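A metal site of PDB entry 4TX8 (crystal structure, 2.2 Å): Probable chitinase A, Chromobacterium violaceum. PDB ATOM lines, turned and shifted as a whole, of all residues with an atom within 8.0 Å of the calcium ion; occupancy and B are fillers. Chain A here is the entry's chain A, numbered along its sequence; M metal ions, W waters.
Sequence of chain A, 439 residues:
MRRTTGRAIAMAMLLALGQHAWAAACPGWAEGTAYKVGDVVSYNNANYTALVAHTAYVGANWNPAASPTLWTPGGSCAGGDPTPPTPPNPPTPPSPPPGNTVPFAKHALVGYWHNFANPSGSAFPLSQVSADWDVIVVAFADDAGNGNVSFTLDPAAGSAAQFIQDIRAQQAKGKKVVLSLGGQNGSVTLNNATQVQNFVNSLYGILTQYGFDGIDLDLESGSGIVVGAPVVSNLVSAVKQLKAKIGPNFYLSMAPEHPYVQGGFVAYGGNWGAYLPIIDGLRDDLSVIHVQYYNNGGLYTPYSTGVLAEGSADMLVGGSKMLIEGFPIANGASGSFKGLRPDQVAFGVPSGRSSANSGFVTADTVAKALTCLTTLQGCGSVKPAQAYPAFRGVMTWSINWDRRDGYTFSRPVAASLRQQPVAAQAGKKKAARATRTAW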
ATOM      1  N   TYR A 112      -4.479  18.829  -2.268  1.00  0.00           N
ATOM      2  CA  TYR A 112      -5.300  20.016  -2.043  1.00  0.00           C
ATOM      3  C   TYR A 112      -6.649  19.915  -2.750  1.00  0.00           C
ATOM      4  O   TYR A 112      -6.724  19.567  -3.923  1.00  0.00           O
ATOM      5  CB  TYR A 112      -4.559  21.269  -2.520  1.00  0.00           C
ATOM      6  CG  TYR A 112      -3.398  21.675  -1.640  1.00  0.00           C
ATOM      7  CD1 TYR A 112      -2.165  21.034  -1.748  1.00  0.00           C
ATOM      8  CD2 TYR A 112      -3.531  22.679  -0.698  1.00  0.00           C
ATOM      9  CE1 TYR A 112      -1.107  21.391  -0.943  1.00  0.00           C
ATOM     10  CE2 TYR A 112      -2.475  23.050   0.117  1.00  0.00           C
ATOM     11  CZ  TYR A 112      -1.263  22.399  -0.011  1.00  0.00           C
ATOM     12  OH  TYR A 112      -0.213  22.762   0.804  1.00  0.00           O
ATOM     13  N   PHE A 140      -8.940  27.552  -0.147  1.00  0.00           N
ATOM     14  CA  PHE A 140      -8.128  28.022   0.966  1.00  0.00           C
ATOM     15  C   PHE A 140      -8.988  28.770   1.980  1.00  0.00           C
ATOM     16  O   PHE A 140     -10.167  29.037   1.731  1.00  0.00           O
ATOM     17  CB  PHE A 140      -7.019  28.966   0.500  1.00  0.00           C
ATOM     18  CG  PHE A 140      -6.029  28.350  -0.431  1.00  0.00           C
ATOM     19  CD1 PHE A 140      -4.882  27.739   0.064  1.00  0.00           C
ATOM     20  CD2 PHE A 140      -6.219  28.399  -1.805  1.00  0.00           C
ATOM     21  CE1 PHE A 140      -3.952  27.173  -0.795  1.00  0.00           C
ATOM     22  CE2 PHE A 140      -5.290  27.833  -2.674  1.00  0.00           C
ATOM     23  CZ  PHE A 140      -4.156  27.220  -2.169  1.00  0.00           C
ATOM     24  N   SER A 180      -6.035  25.102   4.669  1.00  0.00           N
ATOM     25  CA  SER A 180      -4.808  25.740   4.213  1.00  0.00           C
ATOM     26  C   SER A 180      -4.904  27.267   4.185  1.00  0.00           C
ATOM     27  O   SER A 180      -5.907  27.834   3.765  1.00  0.00           O
ATOM     28  CB  SER A 180      -4.423  25.242   2.814  1.00  0.00           C
ATOM     29  OG  SER A 180      -3.211  25.843   2.398  1.00  0.00           O
ATOM     30  N   LEU A 181      -3.840  27.907   4.645  1.00  0.00           N
ATOM     31  CA  LEU A 181      -3.693  29.343   4.529  1.00  0.00           C
ATOM     32  C   LEU A 181      -2.884  29.650   3.273  1.00  0.00           C
ATOM     33  O   LEU A 181      -1.708  29.293   3.192  1.00  0.00           O
ATOM     34  CB  LEU A 181      -2.997  29.922   5.765  1.00  0.00           C
ATOM     35  CG  LEU A 181      -3.814  30.292   7.013  1.00  0.00           C
ATOM     36  CD1 LEU A 181      -4.974  29.339   7.241  1.00  0.00           C
ATOM     37  CD2 LEU A 181      -2.897  30.306   8.218  1.00  0.00           C
ATOM     38  N   GLY A 182      -3.520  30.301   2.307  1.00  0.00           N
ATOM     39  CA  GLY A 182      -2.849  30.625   1.056  1.00  0.00           C
ATOM     40  C   GLY A 182      -3.822  31.089  -0.014  1.00  0.00           C
ATOM     41  O   GLY A 182      -4.918  31.557   0.292  1.00  0.00           O
ATOM     42  N   ASP A 216      -2.635  24.122   7.304  1.00  0.00           N
ATOM     43  CA  ASP A 216      -1.518  24.014   6.382  1.00  0.00           C
ATOM     44  C   ASP A 216      -1.040  25.413   6.033  1.00  0.00           C
ATOM     45  O   ASP A 216      -1.849  26.290   5.722  1.00  0.00           O
ATOM     46  CB  ASP A 216      -1.919  23.246   5.127  1.00  0.00           C
ATOM     47  CG  ASP A 216      -0.827  23.240   4.064  1.00  0.00           C
ATOM     48  OD1 ASP A 216       0.202  22.569   4.274  1.00  0.00           O
ATOM     49  OD2 ASP A 216      -0.998  23.908   3.020  1.00  0.00           O
ATOM     50  N   LEU A 217       0.266  25.645   6.070  1.00  0.00           N
ATOM     51  CA  LEU A 217       0.807  26.944   5.720  1.00  0.00           C
ATOM     52  C   LEU A 217       1.308  26.974   4.279  1.00  0.00           C
ATOM     53  O   LEU A 217       2.340  26.390   3.947  1.00  0.00           O
ATOM     54  CB  LEU A 217       1.936  27.340   6.682  1.00  0.00           C
ATOM     55  CG  LEU A 217       1.584  27.273   8.168  1.00  0.00           C
ATOM     56  CD1 LEU A 217       2.793  27.678   9.006  1.00  0.00           C
ATOM     57  CD2 LEU A 217       0.379  28.155   8.492  1.00  0.00           C
ATOM     58  N   ASP A 218       0.552  27.646   3.418  1.00  0.00           N
ATOM     59  CA  ASP A 218       0.903  27.807   2.021  1.00  0.00           C
ATOM     60  C   ASP A 218       0.822  29.283   1.673  1.00  0.00           C
ATOM     61  O   ASP A 218       0.274  29.674   0.648  1.00  0.00           O
ATOM     62  CB  ASP A 218      -0.040  26.979   1.139  1.00  0.00           C
ATOM     63  CG  ASP A 218       0.392  26.936  -0.319  1.00  0.00           C
ATOM     64  OD1 ASP A 218       1.574  27.199  -0.608  1.00  0.00           O
ATOM     65  OD2 ASP A 218      -0.452  26.627  -1.182  1.00  0.00           O
ATOM     66  N   LEU A 219       1.365  30.116   2.562  1.00  0.00           N
ATOM     67  CA  LEU A 219       1.059  31.553   2.533  1.00  0.00           C
ATOM     68  C   LEU A 219       2.251  32.466   2.274  1.00  0.00           C
ATOM     69  O   LEU A 219       2.120  33.683   2.342  1.00  0.00           O
ATOM     70  CB  LEU A 219       0.405  31.952   3.864  1.00  0.00           C
ATOM     71  CG  LEU A 219       1.014  31.400   5.169  1.00  0.00           C
ATOM     72  CD1 LEU A 219       2.427  31.926   5.438  1.00  0.00           C
ATOM     73  CD2 LEU A 219       0.117  31.702   6.351  1.00  0.00           C
ATOM     74  N   GLU A 220       3.413  31.885   1.997  1.00  0.00           N
ATOM     75  CA  GLU A 220       4.651  32.650   2.039  1.00  0.00           C
ATOM     76  C   GLU A 220       4.773  33.697   0.938  1.00  0.00           C
ATOM     77  O   GLU A 220       5.457  34.706   1.108  1.00  0.00           O
ATOM     78  CB  GLU A 220       5.860  31.714   1.985  1.00  0.00           C
ATOM     79  CG  GLU A 220       6.123  31.072   0.633  1.00  0.00           C
ATOM     80  CD  GLU A 220       5.424  29.734   0.468  1.00  0.00           C
ATOM     81  OE1 GLU A 220       4.439  29.464   1.191  1.00  0.00           O
ATOM     82  OE2 GLU A 220       5.876  28.942  -0.399  1.00  0.00           O
ATOM     83  N   SER A 221       4.113  33.474  -0.194  1.00  0.00           N
ATOM     84  CA  SER A 221       4.351  34.313  -1.356  1.00  0.00           C
ATOM     85  C   SER A 221       3.710  35.687  -1.220  1.00  0.00           C
ATOM     86  O   SER A 221       4.220  36.660  -1.774  1.00  0.00           O
ATOM     87  CB  SER A 221       3.847  33.624  -2.608  1.00  0.00           C
ATOM     88  OG  SER A 221       3.967  34.442  -3.755  1.00  0.00           O
ATOM     89  N   MET A 254       3.310  22.324   6.439  1.00  0.00           N
ATOM     90  CA  MET A 254       3.876  23.474   5.741  1.00  0.00           C
ATOM     91  C   MET A 254       4.180  23.100   4.303  1.00  0.00           C
ATOM     92  O   MET A 254       4.666  22.005   4.029  1.00  0.00           O
ATOM     93  CB  MET A 254       5.155  23.957   6.415  1.00  0.00           C
ATOM     94  CG  MET A 254       5.016  24.281   7.897  1.00  0.00           C
ATOM     95  SD  MET A 254       6.630  24.608   8.611  1.00  0.00           S
ATOM     96  CE  MET A 254       6.180  24.930  10.325  1.00  0.00           C
ATOM     97  N   ALA A 255       3.884  24.009   3.381  1.00  0.00           N
ATOM     98  CA  ALA A 255       4.201  23.766   1.981  1.00  0.00           C
ATOM     99  C   ALA A 255       4.954  24.926   1.335  1.00  0.00           C
ATOM    100  O   ALA A 255       4.485  25.499   0.364  1.00  0.00           O
ATOM    101  CB  ALA A 255       2.914  23.487   1.204  1.00  0.00           C
ATOM    102  N   PRO A 256       6.138  25.261   1.875  1.00  0.00           N
ATOM    103  CA  PRO A 256       6.878  26.370   1.260  1.00  0.00           C
ATOM    104  C   PRO A 256       7.630  25.949   0.006  1.00  0.00           C
ATOM    105  O   PRO A 256       7.987  24.781  -0.141  1.00  0.00           O
ATOM    106  CB  PRO A 256       7.847  26.782   2.368  1.00  0.00           C
ATOM    107  CG  PRO A 256       8.088  25.530   3.127  1.00  0.00           C
ATOM    108  CD  PRO A 256       6.874  24.667   3.006  1.00  0.00           C
ATOM    109  N   GLU A 257       7.843  26.894  -0.906  1.00  0.00           N
ATOM    110  CA  GLU A 257       8.639  26.658  -2.095  1.00  0.00           C
ATOM    111  C   GLU A 257      10.099  26.520  -1.709  1.00  0.00           C
ATOM    112  O   GLU A 257      10.542  27.156  -0.744  1.00  0.00           O
ATOM    113  CB  GLU A 257       8.425  27.790  -3.103  1.00  0.00           C
ATOM    114  CG  GLU A 257       6.955  28.027  -3.410  1.00  0.00           C
ATOM    115  CD  GLU A 257       6.700  29.248  -4.268  1.00  0.00           C
ATOM    116  OE1 GLU A 257       7.434  29.447  -5.260  1.00  0.00           O
ATOM    117  OE2 GLU A 257       5.761  30.000  -3.952  1.00  0.00           O
ATOM    118  N   HIS A 258      10.858  25.713  -2.437  1.00  0.00           N
ATOM    119  CA  HIS A 258      12.194  25.347  -1.953  1.00  0.00           C
ATOM    120  C   HIS A 258      13.200  26.511  -1.808  1.00  0.00           C
ATOM    121  O   HIS A 258      14.103  26.406  -0.981  1.00  0.00           O
ATOM    122  CB  HIS A 258      12.794  24.225  -2.832  1.00  0.00           C
ATOM    123  CG  HIS A 258      13.199  24.635  -4.214  1.00  0.00           C
ATOM    124  ND1 HIS A 258      14.267  25.468  -4.467  1.00  0.00           N
ATOM    125  CD2 HIS A 258      12.727  24.264  -5.432  1.00  0.00           C
ATOM    126  CE1 HIS A 258      14.409  25.617  -5.776  1.00  0.00           C
ATOM    127  NE2 HIS A 258      13.484  24.901  -6.381  1.00  0.00           N
ATOM    128  N   TYR A 260      12.628  29.097  -0.171  1.00  0.00           N
ATOM    129  CA  TYR A 260      12.399  29.537   1.202  1.00  0.00           C
ATOM    130  C   TYR A 260      13.025  28.593   2.232  1.00  0.00           C
ATOM    131  O   TYR A 260      13.170  28.950   3.403  1.00  0.00           O
ATOM    132  CB  TYR A 260      10.905  29.654   1.489  1.00  0.00           C
ATOM    133  CG  TYR A 260      10.205  30.770   0.760  1.00  0.00           C
ATOM    134  CD1 TYR A 260       9.807  30.614  -0.564  1.00  0.00           C
ATOM    135  CD2 TYR A 260       9.933  31.981   1.384  1.00  0.00           C
ATOM    136  CE1 TYR A 260       9.156  31.644  -1.244  1.00  0.00           C
ATOM    137  CE2 TYR A 260       9.290  33.005   0.723  1.00  0.00           C
ATOM    138  CZ  TYR A 260       8.903  32.829  -0.590  1.00  0.00           C
ATOM    139  OH  TYR A 260       8.267  33.847  -1.261  1.00  0.00           O
ATOM    140  N   TYR A 275      12.261  30.706   5.535  1.00  0.00           N
ATOM    141  CA  TYR A 275      11.323  29.844   6.244  1.00  0.00           C
ATOM    142  C   TYR A 275      11.988  28.998   7.331  1.00  0.00           C
ATOM    143  O   TYR A 275      11.299  28.404   8.167  1.00  0.00           O
ATOM    144  CB  TYR A 275      10.602  28.915   5.254  1.00  0.00           C
ATOM    145  CG  TYR A 275       9.120  28.806   5.483  1.00  0.00           C
ATOM    146  CD1 TYR A 275       8.589  27.876   6.357  1.00  0.00           C
ATOM    147  CD2 TYR A 275       8.237  29.635   4.795  1.00  0.00           C
ATOM    148  CE1 TYR A 275       7.227  27.775   6.561  1.00  0.00           C
ATOM    149  CE2 TYR A 275       6.872  29.547   4.989  1.00  0.00           C
ATOM    150  CZ  TYR A 275       6.378  28.615   5.872  1.00  0.00           C
ATOM    151  OH  TYR A 275       5.013  28.527   6.056  1.00  0.00           O
ATOM    152  N   HIS A 290       5.988  19.438   3.394  1.00  0.00           N
ATOM    153  CA  HIS A 290       6.141  18.982   2.023  1.00  0.00           C
ATOM    154  C   HIS A 290       6.475  20.165   1.143  1.00  0.00           C
ATOM    155  O   HIS A 290       5.593  20.888   0.666  1.00  0.00           O
ATOM    156  CB  HIS A 290       4.886  18.261   1.531  1.00  0.00           C
ATOM    157  CG  HIS A 290       3.612  18.766   2.134  1.00  0.00           C
ATOM    158  ND1 HIS A 290       3.210  20.082   2.011  1.00  0.00           N
ATOM    159  CD2 HIS A 290       2.651  18.136   2.840  1.00  0.00           C
ATOM    160  CE1 HIS A 290       2.045  20.238   2.624  1.00  0.00           C
ATOM    161  NE2 HIS A 290       1.687  19.070   3.135  1.00  0.00           N
ATOM    162  N   VAL A 291       7.774  20.379   0.950  1.00  0.00           N
ATOM    163  CA  VAL A 291       8.271  21.476   0.134  1.00  0.00           C
ATOM    164  C   VAL A 291       7.767  21.335  -1.306  1.00  0.00           C
ATOM    165  O   VAL A 291       7.659  20.232  -1.836  1.00  0.00           O
ATOM    166  CB  VAL A 291       9.815  21.525   0.174  1.00  0.00           C
ATOM    167  CG1 VAL A 291      10.388  22.308  -1.000  1.00  0.00           C
ATOM    168  CG2 VAL A 291      10.283  22.132   1.498  1.00  0.00           C
ATOM    169  N   GLN A 292       7.421  22.461  -1.908  1.00  0.00           N
ATOM    170  CA  GLN A 292       6.993  22.465  -3.293  1.00  0.00           C
ATOM    171  C   GLN A 292       8.207  22.448  -4.211  1.00  0.00           C
ATOM    172  O   GLN A 292       8.940  23.432  -4.323  1.00  0.00           O
ATOM    173  CB  GLN A 292       6.098  23.688  -3.566  1.00  0.00           C
ATOM    174  CG  GLN A 292       4.806  23.672  -2.765  1.00  0.00           C
ATOM    175  CD  GLN A 292       4.065  25.003  -2.755  1.00  0.00           C
ATOM    176  OE1 GLN A 292       4.543  26.000  -3.308  1.00  0.00           O
ATOM    177  NE2 GLN A 292       2.894  25.037  -2.140  1.00  0.00           N
ATOM    178  N   TYR A 294       8.400  22.615  -7.373  1.00  0.00           N
ATOM    179  CA  TYR A 294       7.985  23.042  -8.704  1.00  0.00           C
ATOM    180  C   TYR A 294       7.943  24.561  -8.814  1.00  0.00           C
ATOM    181  O   TYR A 294       7.944  25.262  -7.803  1.00  0.00           O
ATOM    182  CB  TYR A 294       6.618  22.450  -9.083  1.00  0.00           C
ATOM    183  CG  TYR A 294       5.553  22.473  -8.002  1.00  0.00           C
ATOM    184  CD1 TYR A 294       5.499  21.469  -7.035  1.00  0.00           C
ATOM    185  CD2 TYR A 294       4.572  23.459  -7.978  1.00  0.00           C
ATOM    186  CE1 TYR A 294       4.526  21.468  -6.056  1.00  0.00           C
ATOM    187  CE2 TYR A 294       3.591  23.464  -6.999  1.00  0.00           C
ATOM    188  CZ  TYR A 294       3.579  22.465  -6.044  1.00  0.00           C
ATOM    189  OH  TYR A 294       2.607  22.450  -5.065  1.00  0.00           O
ATOM    190  N   ASN A 296      10.151  26.606  -9.509  1.00  0.00           N
ATOM    191  CA  ASN A 296      11.321  27.366  -9.044  1.00  0.00           C
ATOM    192  C   ASN A 296      12.661  26.827  -9.549  1.00  0.00           C
ATOM    193  O   ASN A 296      13.702  27.073  -8.942  1.00  0.00           O
ATOM    194  CB  ASN A 296      11.325  27.430  -7.514  1.00  0.00           C
ATOM    195  CG  ASN A 296      10.250  28.360  -6.975  1.00  0.00           C
ATOM    196  OD1 ASN A 296      10.447  29.576  -6.910  1.00  0.00           O
ATOM    197  ND2 ASN A 296       9.110  27.803  -6.593  1.00  0.00           N
ATOM    198  N   MET A 395       3.065  14.935  -1.434  1.00  0.00           N
ATOM    199  CA  MET A 395       2.019  15.940  -1.558  1.00  0.00           C
ATOM    200  C   MET A 395       1.850  16.347  -3.018  1.00  0.00           C
ATOM    201  O   MET A 395       2.829  16.380  -3.767  1.00  0.00           O
ATOM    202  CB  MET A 395       2.338  17.172  -0.697  1.00  0.00           C
ATOM    203  CG  MET A 395       1.369  18.344  -0.856  1.00  0.00           C
ATOM    204  SD  MET A 395       1.721  19.439  -2.266  1.00  0.00           S
ATOM    205  CE  MET A 395       2.756  20.683  -1.493  1.00  0.00           C
HETATM  206 CA    CA M   1       3.908  27.648  -0.575  1.00  0.00          CA
HETATM  207  O   HOH W   1       3.348  29.026  -2.644  1.00  0.00           O
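The calcium ion is bound by OE2 of Glu 220 (2.4 Å), OD1 of Asp 218 (2.4 Å), O of Ala 255 (2.4 Å), water W1 (2.5 Å) and OE1 of Glu 220 (2.6 Å). The calcium ion has five donor atoms within binding distance.
Water W1 bridges the side-chain carboxylate of Glu 257 (2.9 Å) and the side-chain amide oxygen of Gln 292 (3.3 Å).
Merely in contact with the calcium ion: Pro 256 and Gln 292. Five residues have an atom within 4 Å of the calcium ion: Asp 218, Glu 220, Ala 255, Pro 256 and Gln 292.
OE2 of Glu 220 sits close to N of Glu 257 (2.9 Å). The side-chain carboxylate (OD1) of Asp 218 sits close to the side-chain amide nitrogen (NE2) of Gln 292, 3.0 Å away. The backbone NH of Asp 218 sits at hydrogen-bond distance from the backbone carbonyl oxygen of Leu 181. NE2 of Gln 292 sits close to O of Ala 255 (3.0 Å). The backbone carbonyl oxygen of Leu 217 lies within hydrogen-bond range of the backbone NH of Ala 255 (2.9 Å). N of Gln 292 lies within hydrogen-bond range of O of Pro 256 (3.0 Å).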
